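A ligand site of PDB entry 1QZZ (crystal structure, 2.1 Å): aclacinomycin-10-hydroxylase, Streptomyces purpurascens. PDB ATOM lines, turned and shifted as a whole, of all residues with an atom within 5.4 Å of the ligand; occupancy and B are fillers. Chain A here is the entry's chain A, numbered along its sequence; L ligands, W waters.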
ATOM      1  N   TRP A 146     -10.352 -20.231   1.023  1.00  0.00           N
ATOM      2  CA  TRP A 146     -11.357 -21.122   0.425  1.00  0.00           C
ATOM      3  C   TRP A 146     -11.066 -22.620   0.561  1.00  0.00           C
ATOM      4  O   TRP A 146     -11.982 -23.400   0.719  1.00  0.00           O
ATOM      5  CB  TRP A 146     -11.651 -20.742  -0.999  1.00  0.00           C
ATOM      6  CG  TRP A 146     -12.214 -19.369  -1.073  1.00  0.00           C
ATOM      7  CD1 TRP A 146     -11.613 -18.261  -1.581  1.00  0.00           C
ATOM      8  CD2 TRP A 146     -13.495 -18.943  -0.611  1.00  0.00           C
ATOM      9  NE1 TRP A 146     -12.435 -17.171  -1.464  1.00  0.00           N
ATOM     10  CE2 TRP A 146     -13.601 -17.574  -0.868  1.00  0.00           C
ATOM     11  CE3 TRP A 146     -14.571 -19.595  -0.003  1.00  0.00           C
ATOM     12  CZ2 TRP A 146     -14.746 -16.837  -0.545  1.00  0.00           C
ATOM     13  CZ3 TRP A 146     -15.697 -18.870   0.319  1.00  0.00           C
ATOM     14  CH2 TRP A 146     -15.780 -17.506   0.043  1.00  0.00           C
ATOM     15  N   CYS A 165     -26.295 -13.404   0.741  1.00  0.00           N
ATOM     16  CA  CYS A 165     -26.381 -14.258  -0.443  1.00  0.00           C
ATOM     17  C   CYS A 165     -26.855 -15.666  -0.120  1.00  0.00           C
ATOM     18  O   CYS A 165     -27.398 -16.366  -0.978  1.00  0.00           O
ATOM     19  CB  CYS A 165     -25.044 -14.319  -1.192  1.00  0.00           C
ATOM     20  SG  CYS A 165     -24.728 -12.861  -2.211  1.00  0.00           S
ATOM     21  N   TYR A 171     -31.075 -14.875  -4.835  1.00  0.00           N
ATOM     22  CA  TYR A 171     -30.740 -14.787  -6.245  1.00  0.00           C
ATOM     23  C   TYR A 171     -31.910 -14.496  -7.202  1.00  0.00           C
ATOM     24  O   TYR A 171     -31.724 -14.422  -8.409  1.00  0.00           O
ATOM     25  CB  TYR A 171     -30.008 -16.073  -6.671  1.00  0.00           C
ATOM     26  CG  TYR A 171     -28.666 -16.228  -5.998  1.00  0.00           C
ATOM     27  CD1 TYR A 171     -28.522 -16.997  -4.857  1.00  0.00           C
ATOM     28  CD2 TYR A 171     -27.551 -15.586  -6.504  1.00  0.00           C
ATOM     29  CE1 TYR A 171     -27.283 -17.124  -4.237  1.00  0.00           C
ATOM     30  CE2 TYR A 171     -26.318 -15.719  -5.921  1.00  0.00           C
ATOM     31  CZ  TYR A 171     -26.185 -16.473  -4.776  1.00  0.00           C
ATOM     32  OH  TYR A 171     -24.954 -16.582  -4.195  1.00  0.00           O
ATOM     33  N   ASP A 188     -20.935 -22.705 -14.455  1.00  0.00           N
ATOM     34  CA  ASP A 188     -20.981 -21.899 -13.238  1.00  0.00           C
ATOM     35  C   ASP A 188     -19.666 -22.111 -12.506  1.00  0.00           C
ATOM     36  O   ASP A 188     -19.518 -23.030 -11.703  1.00  0.00           O
ATOM     37  CB  ASP A 188     -22.196 -22.377 -12.419  1.00  0.00           C
ATOM     38  CG  ASP A 188     -22.475 -21.531 -11.200  1.00  0.00           C
ATOM     39  OD1 ASP A 188     -21.927 -20.404 -11.072  1.00  0.00           O
ATOM     40  OD2 ASP A 188     -23.252 -21.927 -10.308  1.00  0.00           O
ATOM     41  N   VAL A 189     -18.704 -21.230 -12.800  1.00  0.00           N
ATOM     42  CA  VAL A 189     -17.330 -21.326 -12.284  1.00  0.00           C
ATOM     43  C   VAL A 189     -17.227 -20.820 -10.835  1.00  0.00           C
ATOM     44  O   VAL A 189     -17.423 -19.651 -10.566  1.00  0.00           O
ATOM     45  CB  VAL A 189     -16.377 -20.531 -13.210  1.00  0.00           C
ATOM     46  CG1 VAL A 189     -14.926 -20.636 -12.747  1.00  0.00           C
ATOM     47  CG2 VAL A 189     -16.522 -20.985 -14.690  1.00  0.00           C
ATOM     48  N   GLY A 190     -16.887 -21.713  -9.909  1.00  0.00           N
ATOM     49  CA  GLY A 190     -16.854 -21.355  -8.498  1.00  0.00           C
ATOM     50  C   GLY A 190     -18.255 -21.006  -8.055  1.00  0.00           C
ATOM     51  O   GLY A 190     -18.477 -20.006  -7.366  1.00  0.00           O
ATOM     52  N   GLY A 191     -19.216 -21.842  -8.450  1.00  0.00           N
ATOM     53  CA  GLY A 191     -20.601 -21.553  -8.169  1.00  0.00           C
ATOM     54  C   GLY A 191     -21.059 -21.709  -6.721  1.00  0.00           C
ATOM     55  O   GLY A 191     -22.231 -21.535  -6.441  1.00  0.00           O
ATOM     56  N   GLY A 192     -20.153 -22.019  -5.812  1.00  0.00           N
ATOM     57  CA  GLY A 192     -20.528 -22.208  -4.403  1.00  0.00           C
ATOM     58  C   GLY A 192     -21.557 -23.329  -4.266  1.00  0.00           C
ATOM     59  O   GLY A 192     -21.410 -24.372  -4.889  1.00  0.00           O
ATOM     60  N   MET A 196     -27.327 -19.235  -7.482  1.00  0.00           N
ATOM     61  CA  MET A 196     -27.645 -18.564  -8.748  1.00  0.00           C
ATOM     62  C   MET A 196     -28.045 -19.555  -9.839  1.00  0.00           C
ATOM     63  O   MET A 196     -29.022 -19.355 -10.542  1.00  0.00           O
ATOM     64  CB  MET A 196     -26.480 -17.685  -9.231  1.00  0.00           C
ATOM     65  CG  MET A 196     -26.777 -16.902 -10.495  1.00  0.00           C
ATOM     66  SD  MET A 196     -28.139 -15.770 -10.229  1.00  0.00           S
ATOM     67  CE  MET A 196     -28.284 -14.987 -11.832  1.00  0.00           C
ATOM     68  N   VAL A 212     -18.644 -25.898 -11.249  1.00  0.00           N
ATOM     69  CA  VAL A 212     -17.284 -26.279 -10.864  1.00  0.00           C
ATOM     70  C   VAL A 212     -16.945 -25.654  -9.498  1.00  0.00           C
ATOM     71  O   VAL A 212     -17.022 -24.431  -9.326  1.00  0.00           O
ATOM     72  CB  VAL A 212     -16.247 -25.809 -11.895  1.00  0.00           C
ATOM     73  CG1 VAL A 212     -14.851 -26.008 -11.348  1.00  0.00           C
ATOM     74  CG2 VAL A 212     -16.443 -26.534 -13.259  1.00  0.00           C
ATOM     75  N   GLU A 213     -16.532 -26.481  -8.544  1.00  0.00           N
ATOM     76  CA  GLU A 213     -16.277 -26.021  -7.191  1.00  0.00           C
ATOM     77  C   GLU A 213     -15.267 -26.928  -6.475  1.00  0.00           C
ATOM     78  O   GLU A 213     -14.947 -28.010  -6.959  1.00  0.00           O
ATOM     79  CB  GLU A 213     -17.562 -26.051  -6.380  1.00  0.00           C
ATOM     80  CG  GLU A 213     -18.200 -24.697  -6.128  1.00  0.00           C
ATOM     81  CD  GLU A 213     -17.310 -23.774  -5.325  1.00  0.00           C
ATOM     82  OE1 GLU A 213     -16.384 -24.264  -4.631  1.00  0.00           O
ATOM     83  OE2 GLU A 213     -17.538 -22.547  -5.387  1.00  0.00           O
ATOM     84  N   LEU A 214     -14.799 -26.462  -5.317  1.00  0.00           N
ATOM     85  CA  LEU A 214     -13.965 -27.262  -4.411  1.00  0.00           C
ATOM     86  C   LEU A 214     -14.901 -28.308  -3.771  1.00  0.00           C
ATOM     87  O   LEU A 214     -16.115 -28.194  -3.870  1.00  0.00           O
ATOM     88  CB  LEU A 214     -13.309 -26.350  -3.353  1.00  0.00           C
ATOM     89  CG  LEU A 214     -12.358 -25.243  -3.848  1.00  0.00           C
ATOM     90  CD1 LEU A 214     -11.694 -24.513  -2.672  1.00  0.00           C
ATOM     91  CD2 LEU A 214     -11.290 -25.790  -4.810  1.00  0.00           C
ATOM     92  N   PRO A 217     -18.199 -26.946  -1.064  1.00  0.00           N
ATOM     93  CA  PRO A 217     -19.380 -26.368  -1.709  1.00  0.00           C
ATOM     94  C   PRO A 217     -19.980 -27.319  -2.760  1.00  0.00           C
ATOM     95  O   PRO A 217     -21.188 -27.301  -2.947  1.00  0.00           O
ATOM     96  CB  PRO A 217     -18.839 -25.094  -2.363  1.00  0.00           C
ATOM     97  CG  PRO A 217     -17.572 -24.815  -1.607  1.00  0.00           C
ATOM     98  CD  PRO A 217     -16.995 -26.136  -1.251  1.00  0.00           C
ATOM     99  N   GLY A 239     -13.593 -29.300  -9.034  1.00  0.00           N
ATOM    100  CA  GLY A 239     -12.496 -28.828  -9.857  1.00  0.00           C
ATOM    101  C   GLY A 239     -11.791 -27.590  -9.341  1.00  0.00           C
ATOM    102  O   GLY A 239     -12.232 -26.949  -8.395  1.00  0.00           O
ATOM    103  N   ASP A 240     -10.695 -27.257  -9.999  1.00  0.00           N
ATOM    104  CA  ASP A 240      -9.882 -26.111  -9.616  1.00  0.00           C
ATOM    105  C   ASP A 240      -9.978 -25.123 -10.763  1.00  0.00           C
ATOM    106  O   ASP A 240      -9.480 -25.387 -11.839  1.00  0.00           O
ATOM    107  CB  ASP A 240      -8.433 -26.594  -9.426  1.00  0.00           C
ATOM    108  CG  ASP A 240      -7.476 -25.476  -9.089  1.00  0.00           C
ATOM    109  OD1 ASP A 240      -7.890 -24.289  -8.997  1.00  0.00           O
ATOM    110  OD2 ASP A 240      -6.263 -25.701  -8.892  1.00  0.00           O
ATOM    111  N   PHE A 241     -10.632 -23.993 -10.544  1.00  0.00           N
ATOM    112  CA  PHE A 241     -10.813 -23.062 -11.642  1.00  0.00           C
ATOM    113  C   PHE A 241      -9.546 -22.350 -12.114  1.00  0.00           C
ATOM    114  O   PHE A 241      -9.596 -21.506 -12.991  1.00  0.00           O
ATOM    115  CB  PHE A 241     -12.011 -22.120 -11.448  1.00  0.00           C
ATOM    116  CG  PHE A 241     -11.930 -21.215 -10.235  1.00  0.00           C
ATOM    117  CD1 PHE A 241     -10.716 -20.743  -9.765  1.00  0.00           C
ATOM    118  CD2 PHE A 241     -13.100 -20.804  -9.605  1.00  0.00           C
ATOM    119  CE1 PHE A 241     -10.680 -19.890  -8.666  1.00  0.00           C
ATOM    120  CE2 PHE A 241     -13.067 -19.963  -8.512  1.00  0.00           C
ATOM    121  CZ  PHE A 241     -11.855 -19.495  -8.033  1.00  0.00           C
ATOM    122  N   PHE A 242      -8.406 -22.732 -11.523  1.00  0.00           N
ATOM    123  CA  PHE A 242      -7.109 -22.291 -12.014  1.00  0.00           C
ATOM    124  C   PHE A 242      -6.586 -23.224 -13.108  1.00  0.00           C
ATOM    125  O   PHE A 242      -5.654 -22.873 -13.836  1.00  0.00           O
ATOM    126  CB  PHE A 242      -6.096 -22.140 -10.879  1.00  0.00           C
ATOM    127  CG  PHE A 242      -6.333 -20.938 -10.051  1.00  0.00           C
ATOM    128  CD1 PHE A 242      -6.876 -21.043  -8.796  1.00  0.00           C
ATOM    129  CD2 PHE A 242      -6.092 -19.699 -10.581  1.00  0.00           C
ATOM    130  CE1 PHE A 242      -7.111 -19.929  -8.055  1.00  0.00           C
ATOM    131  CE2 PHE A 242      -6.338 -18.569  -9.836  1.00  0.00           C
ATOM    132  CZ  PHE A 242      -6.862 -18.685  -8.582  1.00  0.00           C
ATOM    133  N   SER A 255     -20.271 -15.733 -10.492  1.00  0.00           N
ATOM    134  CA  SER A 255     -21.169 -15.097  -9.529  1.00  0.00           C
ATOM    135  C   SER A 255     -20.458 -14.850  -8.210  1.00  0.00           C
ATOM    136  O   SER A 255     -20.155 -15.787  -7.460  1.00  0.00           O
ATOM    137  CB  SER A 255     -22.433 -15.970  -9.345  1.00  0.00           C
ATOM    138  OG  SER A 255     -23.269 -15.494  -8.310  1.00  0.00           O
ATOM    139  N   PHE A 256     -20.159 -13.579  -7.946  1.00  0.00           N
ATOM    140  CA  PHE A 256     -19.387 -13.225  -6.749  1.00  0.00           C
ATOM    141  C   PHE A 256     -18.135 -14.076  -6.605  1.00  0.00           C
ATOM    142  O   PHE A 256     -17.895 -14.673  -5.554  1.00  0.00           O
ATOM    143  CB  PHE A 256     -20.279 -13.286  -5.481  1.00  0.00           C
ATOM    144  CG  PHE A 256     -21.488 -12.426  -5.592  1.00  0.00           C
ATOM    145  CD1 PHE A 256     -22.696 -12.952  -6.027  1.00  0.00           C
ATOM    146  CD2 PHE A 256     -21.407 -11.067  -5.338  1.00  0.00           C
ATOM    147  CE1 PHE A 256     -23.804 -12.140  -6.168  1.00  0.00           C
ATOM    148  CE2 PHE A 256     -22.514 -10.254  -5.479  1.00  0.00           C
ATOM    149  CZ  PHE A 256     -23.711 -10.787  -5.903  1.00  0.00           C
ATOM    150  N   VAL A 257     -17.323 -14.133  -7.661  1.00  0.00           N
ATOM    151  CA  VAL A 257     -16.050 -14.848  -7.614  1.00  0.00           C
ATOM    152  C   VAL A 257     -14.830 -13.909  -7.782  1.00  0.00           C
ATOM    153  O   VAL A 257     -13.848 -13.982  -7.030  1.00  0.00           O
ATOM    154  CB  VAL A 257     -15.956 -15.965  -8.688  1.00  0.00           C
ATOM    155  CG1 VAL A 257     -14.570 -16.530  -8.736  1.00  0.00           C
ATOM    156  CG2 VAL A 257     -16.987 -17.078  -8.439  1.00  0.00           C
ATOM    157  N   LEU A 259     -14.207 -10.755  -7.127  1.00  0.00           N
ATOM    158  CA  LEU A 259     -13.892  -9.935  -5.976  1.00  0.00           C
ATOM    159  C   LEU A 259     -13.025 -10.671  -4.941  1.00  0.00           C
ATOM    160  O   LEU A 259     -12.429 -10.047  -4.079  1.00  0.00           O
ATOM    161  CB  LEU A 259     -15.202  -9.429  -5.316  1.00  0.00           C
ATOM    162  CG  LEU A 259     -15.877 -10.362  -4.311  1.00  0.00           C
ATOM    163  CD1 LEU A 259     -16.954  -9.650  -3.496  1.00  0.00           C
ATOM    164  CD2 LEU A 259     -16.446 -11.599  -5.007  1.00  0.00           C
ATOM    165  N   ASN A 260     -12.987 -12.007  -5.011  1.00  0.00           N
ATOM    166  CA  ASN A 260     -12.172 -12.781  -4.066  1.00  0.00           C
ATOM    167  C   ASN A 260     -10.709 -12.882  -4.501  1.00  0.00           C
ATOM    168  O   ASN A 260      -9.906 -13.507  -3.795  1.00  0.00           O
ATOM    169  CB  ASN A 260     -12.653 -14.233  -3.935  1.00  0.00           C
ATOM    170  CG  ASN A 260     -14.028 -14.370  -3.290  1.00  0.00           C
ATOM    171  OD1 ASN A 260     -14.767 -15.292  -3.629  1.00  0.00           O
ATOM    172  ND2 ASN A 260     -14.350 -13.514  -2.337  1.00  0.00           N
ATOM    173  N   TRP A 261     -10.361 -12.309  -5.640  1.00  0.00           N
ATOM    174  CA  TRP A 261      -9.021 -12.538  -6.190  1.00  0.00           C
ATOM    175  C   TRP A 261      -8.250 -11.302  -6.606  1.00  0.00           C
ATOM    176  O   TRP A 261      -8.834 -10.307  -7.054  1.00  0.00           O
ATOM    177  CB  TRP A 261      -9.119 -13.524  -7.372  1.00  0.00           C
ATOM    178  CG  TRP A 261      -9.688 -14.834  -6.955  1.00  0.00           C
ATOM    179  CD1 TRP A 261     -10.983 -15.259  -7.086  1.00  0.00           C
ATOM    180  CD2 TRP A 261      -8.996 -15.884  -6.278  1.00  0.00           C
ATOM    181  NE1 TRP A 261     -11.136 -16.517  -6.535  1.00  0.00           N
ATOM    182  CE2 TRP A 261      -9.920 -16.933  -6.050  1.00  0.00           C
ATOM    183  CE3 TRP A 261      -7.678 -16.068  -5.860  1.00  0.00           C
ATOM    184  CZ2 TRP A 261      -9.567 -18.128  -5.419  1.00  0.00           C
ATOM    185  CZ3 TRP A 261      -7.332 -17.258  -5.217  1.00  0.00           C
ATOM    186  CH2 TRP A 261      -8.273 -18.264  -5.009  1.00  0.00           C
HETATM  187  N1  LIG L   1     -20.775 -18.541  -7.018  1.00  0.00           N
HETATM  188  C1  LIG L   1     -20.911 -18.309  -5.557  1.00  0.00           C
HETATM  189  C2  LIG L   1     -22.043 -17.333  -5.273  1.00  0.00           C
HETATM  190  O1  LIG L   1     -22.902 -17.079  -6.128  1.00  0.00           O
HETATM  191  O2  LIG L   1     -22.020 -16.799  -4.112  1.00  0.00           O
HETATM  192  C3  LIG L   1     -19.599 -17.803  -4.957  1.00  0.00           C
HETATM  193  C4  LIG L   1     -19.312 -18.415  -3.610  1.00  0.00           C
HETATM  194  S1  LIG L   1     -17.877 -17.645  -2.789  1.00  0.00           S
HETATM  195  C5  LIG L   1     -18.065 -15.871  -2.964  1.00  0.00           C
HETATM  196  C6  LIG L   1     -16.554 -18.055  -3.910  1.00  0.00           C
HETATM  197  C7  LIG L   1     -16.409 -19.511  -4.308  1.00  0.00           C
HETATM  198  O3  LIG L   1     -15.190 -19.736  -5.108  1.00  0.00           O
HETATM  199  C8  LIG L   1     -16.329 -20.392  -3.037  1.00  0.00           C
HETATM  200  O4  LIG L   1     -17.423 -21.323  -3.005  1.00  0.00           O
HETATM  201  C9  LIG L   1     -15.020 -21.176  -3.215  1.00  0.00           C
HETATM  202  O5  LIG L   1     -15.090 -22.555  -2.845  1.00  0.00           O
HETATM  203  C10 LIG L   1     -14.827 -21.023  -4.727  1.00  0.00           C
HETATM  204  N2  LIG L   1     -13.457 -21.281  -5.075  1.00  0.00           N
HETATM  205  C11 LIG L   1     -12.331 -20.698  -4.548  1.00  0.00           C
HETATM  206  N3  LIG L   1     -11.281 -21.197  -5.148  1.00  0.00           N
HETATM  207  C12 LIG L   1     -11.683 -22.127  -6.087  1.00  0.00           C
HETATM  208  C13 LIG L   1     -11.005 -22.959  -7.015  1.00  0.00           C
HETATM  209  N4  LIG L   1      -9.656 -22.969  -7.122  1.00  0.00           N
HETATM  210  N5  LIG L   1     -11.740 -23.774  -7.780  1.00  0.00           N
HETATM  211  C14 LIG L   1     -13.055 -23.735  -7.644  1.00  0.00           C
HETATM  212  N6  LIG L   1     -13.776 -22.971  -6.815  1.00  0.00           N
HETATM  213  C15 LIG L   1     -13.042 -22.174  -6.024  1.00  0.00           C
HETATM  214  O   HOH W   1     -13.517 -17.333  -5.387  1.00  0.00           O
HETATM  215  O   HOH W   2     -18.975 -21.154  -0.966  1.00  0.00           O
HETATM  216  O   HOH W   3     -19.917 -18.569 -10.097  1.00  0.00           O
HETATM  217  O   HOH W   4     -14.777 -23.304  -0.153  1.00  0.00           O
HETATM  218  O   HOH W   5     -22.491 -14.507  -2.693  1.00  0.00           O
HETATM  219  O   HOH W   6     -19.636 -16.448  -0.492  1.00  0.00           O
HETATM  220  O   HOH W   7      -7.056 -21.802  -5.250  1.00  0.00           O
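OE2 of Glu 213 sits at hydrogen-bond distance from O4 of the ligand (2.7 Å).
A nitrogen (N1) of the ligand is in hydrogen-bond range of the backbone carbonyl oxygen (O) of Ser 255, 2.9 Å away.
O1 of the ligand is in hydrogen-bond range of OG of Ser 255 (2.7 Å).
N1 of the ligand sits at hydrogen-bond distance from O of Gly 190.
O1 of the ligand sits at hydrogen-bond distance from OH of Tyr 171 (2.9 Å).
A nitrogen (N4) of the ligand is in hydrogen-bond range of the side-chain carboxylate of Asp 240 (2.9 Å).
A nitrogen (N5) of the ligand is in hydrogen-bond range of the backbone NH (N) of Phe 241 (3.0 Å).
The backbone carbonyl oxygen (O) of Gly 191 lies close to a nitrogen (N1) of the ligand (3.4 Å).
N5 of the ligand sits close to O of Gly 239 (3.3 Å).
Residues that only touch the ligand: Trp 146 (3.5 Å), Gly 192 (3.5 Å), Leu 214 (3.6 Å), Pro 217 (3.6 Å), Phe 242 (3.8 Å), Phe 256 (2.9 Å), Asn 260 (3.3 Å) and Trp 261 (3.5 Å).
Hydrophobic or aromatic side chains that line the ligand: Trp 146, Tyr 171, Leu 214, Pro 217, Phe 241, Phe 242 and Trp 261.
The nearest printed residue that does not touch the ligand is Val 257 (4.3 Å).
The backbone carbonyl oxygen (O) of Glu 213 is in hydrogen-bond range of the backbone NH (N) of Gly 239.
The backbone NH (N) of Gly 192 is in hydrogen-bond range of the side-chain carboxylate (OE2) of Glu 213.
The backbone NH (N) of Gly 190 lies within hydrogen-bond range of the backbone carbonyl oxygen (O) of Val 212 (2.8 Å).
OD1 of Asp 240 sits close to N of Phe 242, 3.0 Å away.
Water W5 bridges an oxygen (O2) of the ligand (2.7 Å) and the side-chain sulfur (SG) of Cys 165 (2.8 Å).
Water W4 bridges O5 of the ligand (2.8 Å) and O of Trp 146 (2.9 Å).
Water W1 lies within hydrogen-bond range of NE1 of Trp 261, O3 of the ligand and OD1 of Asn 260.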
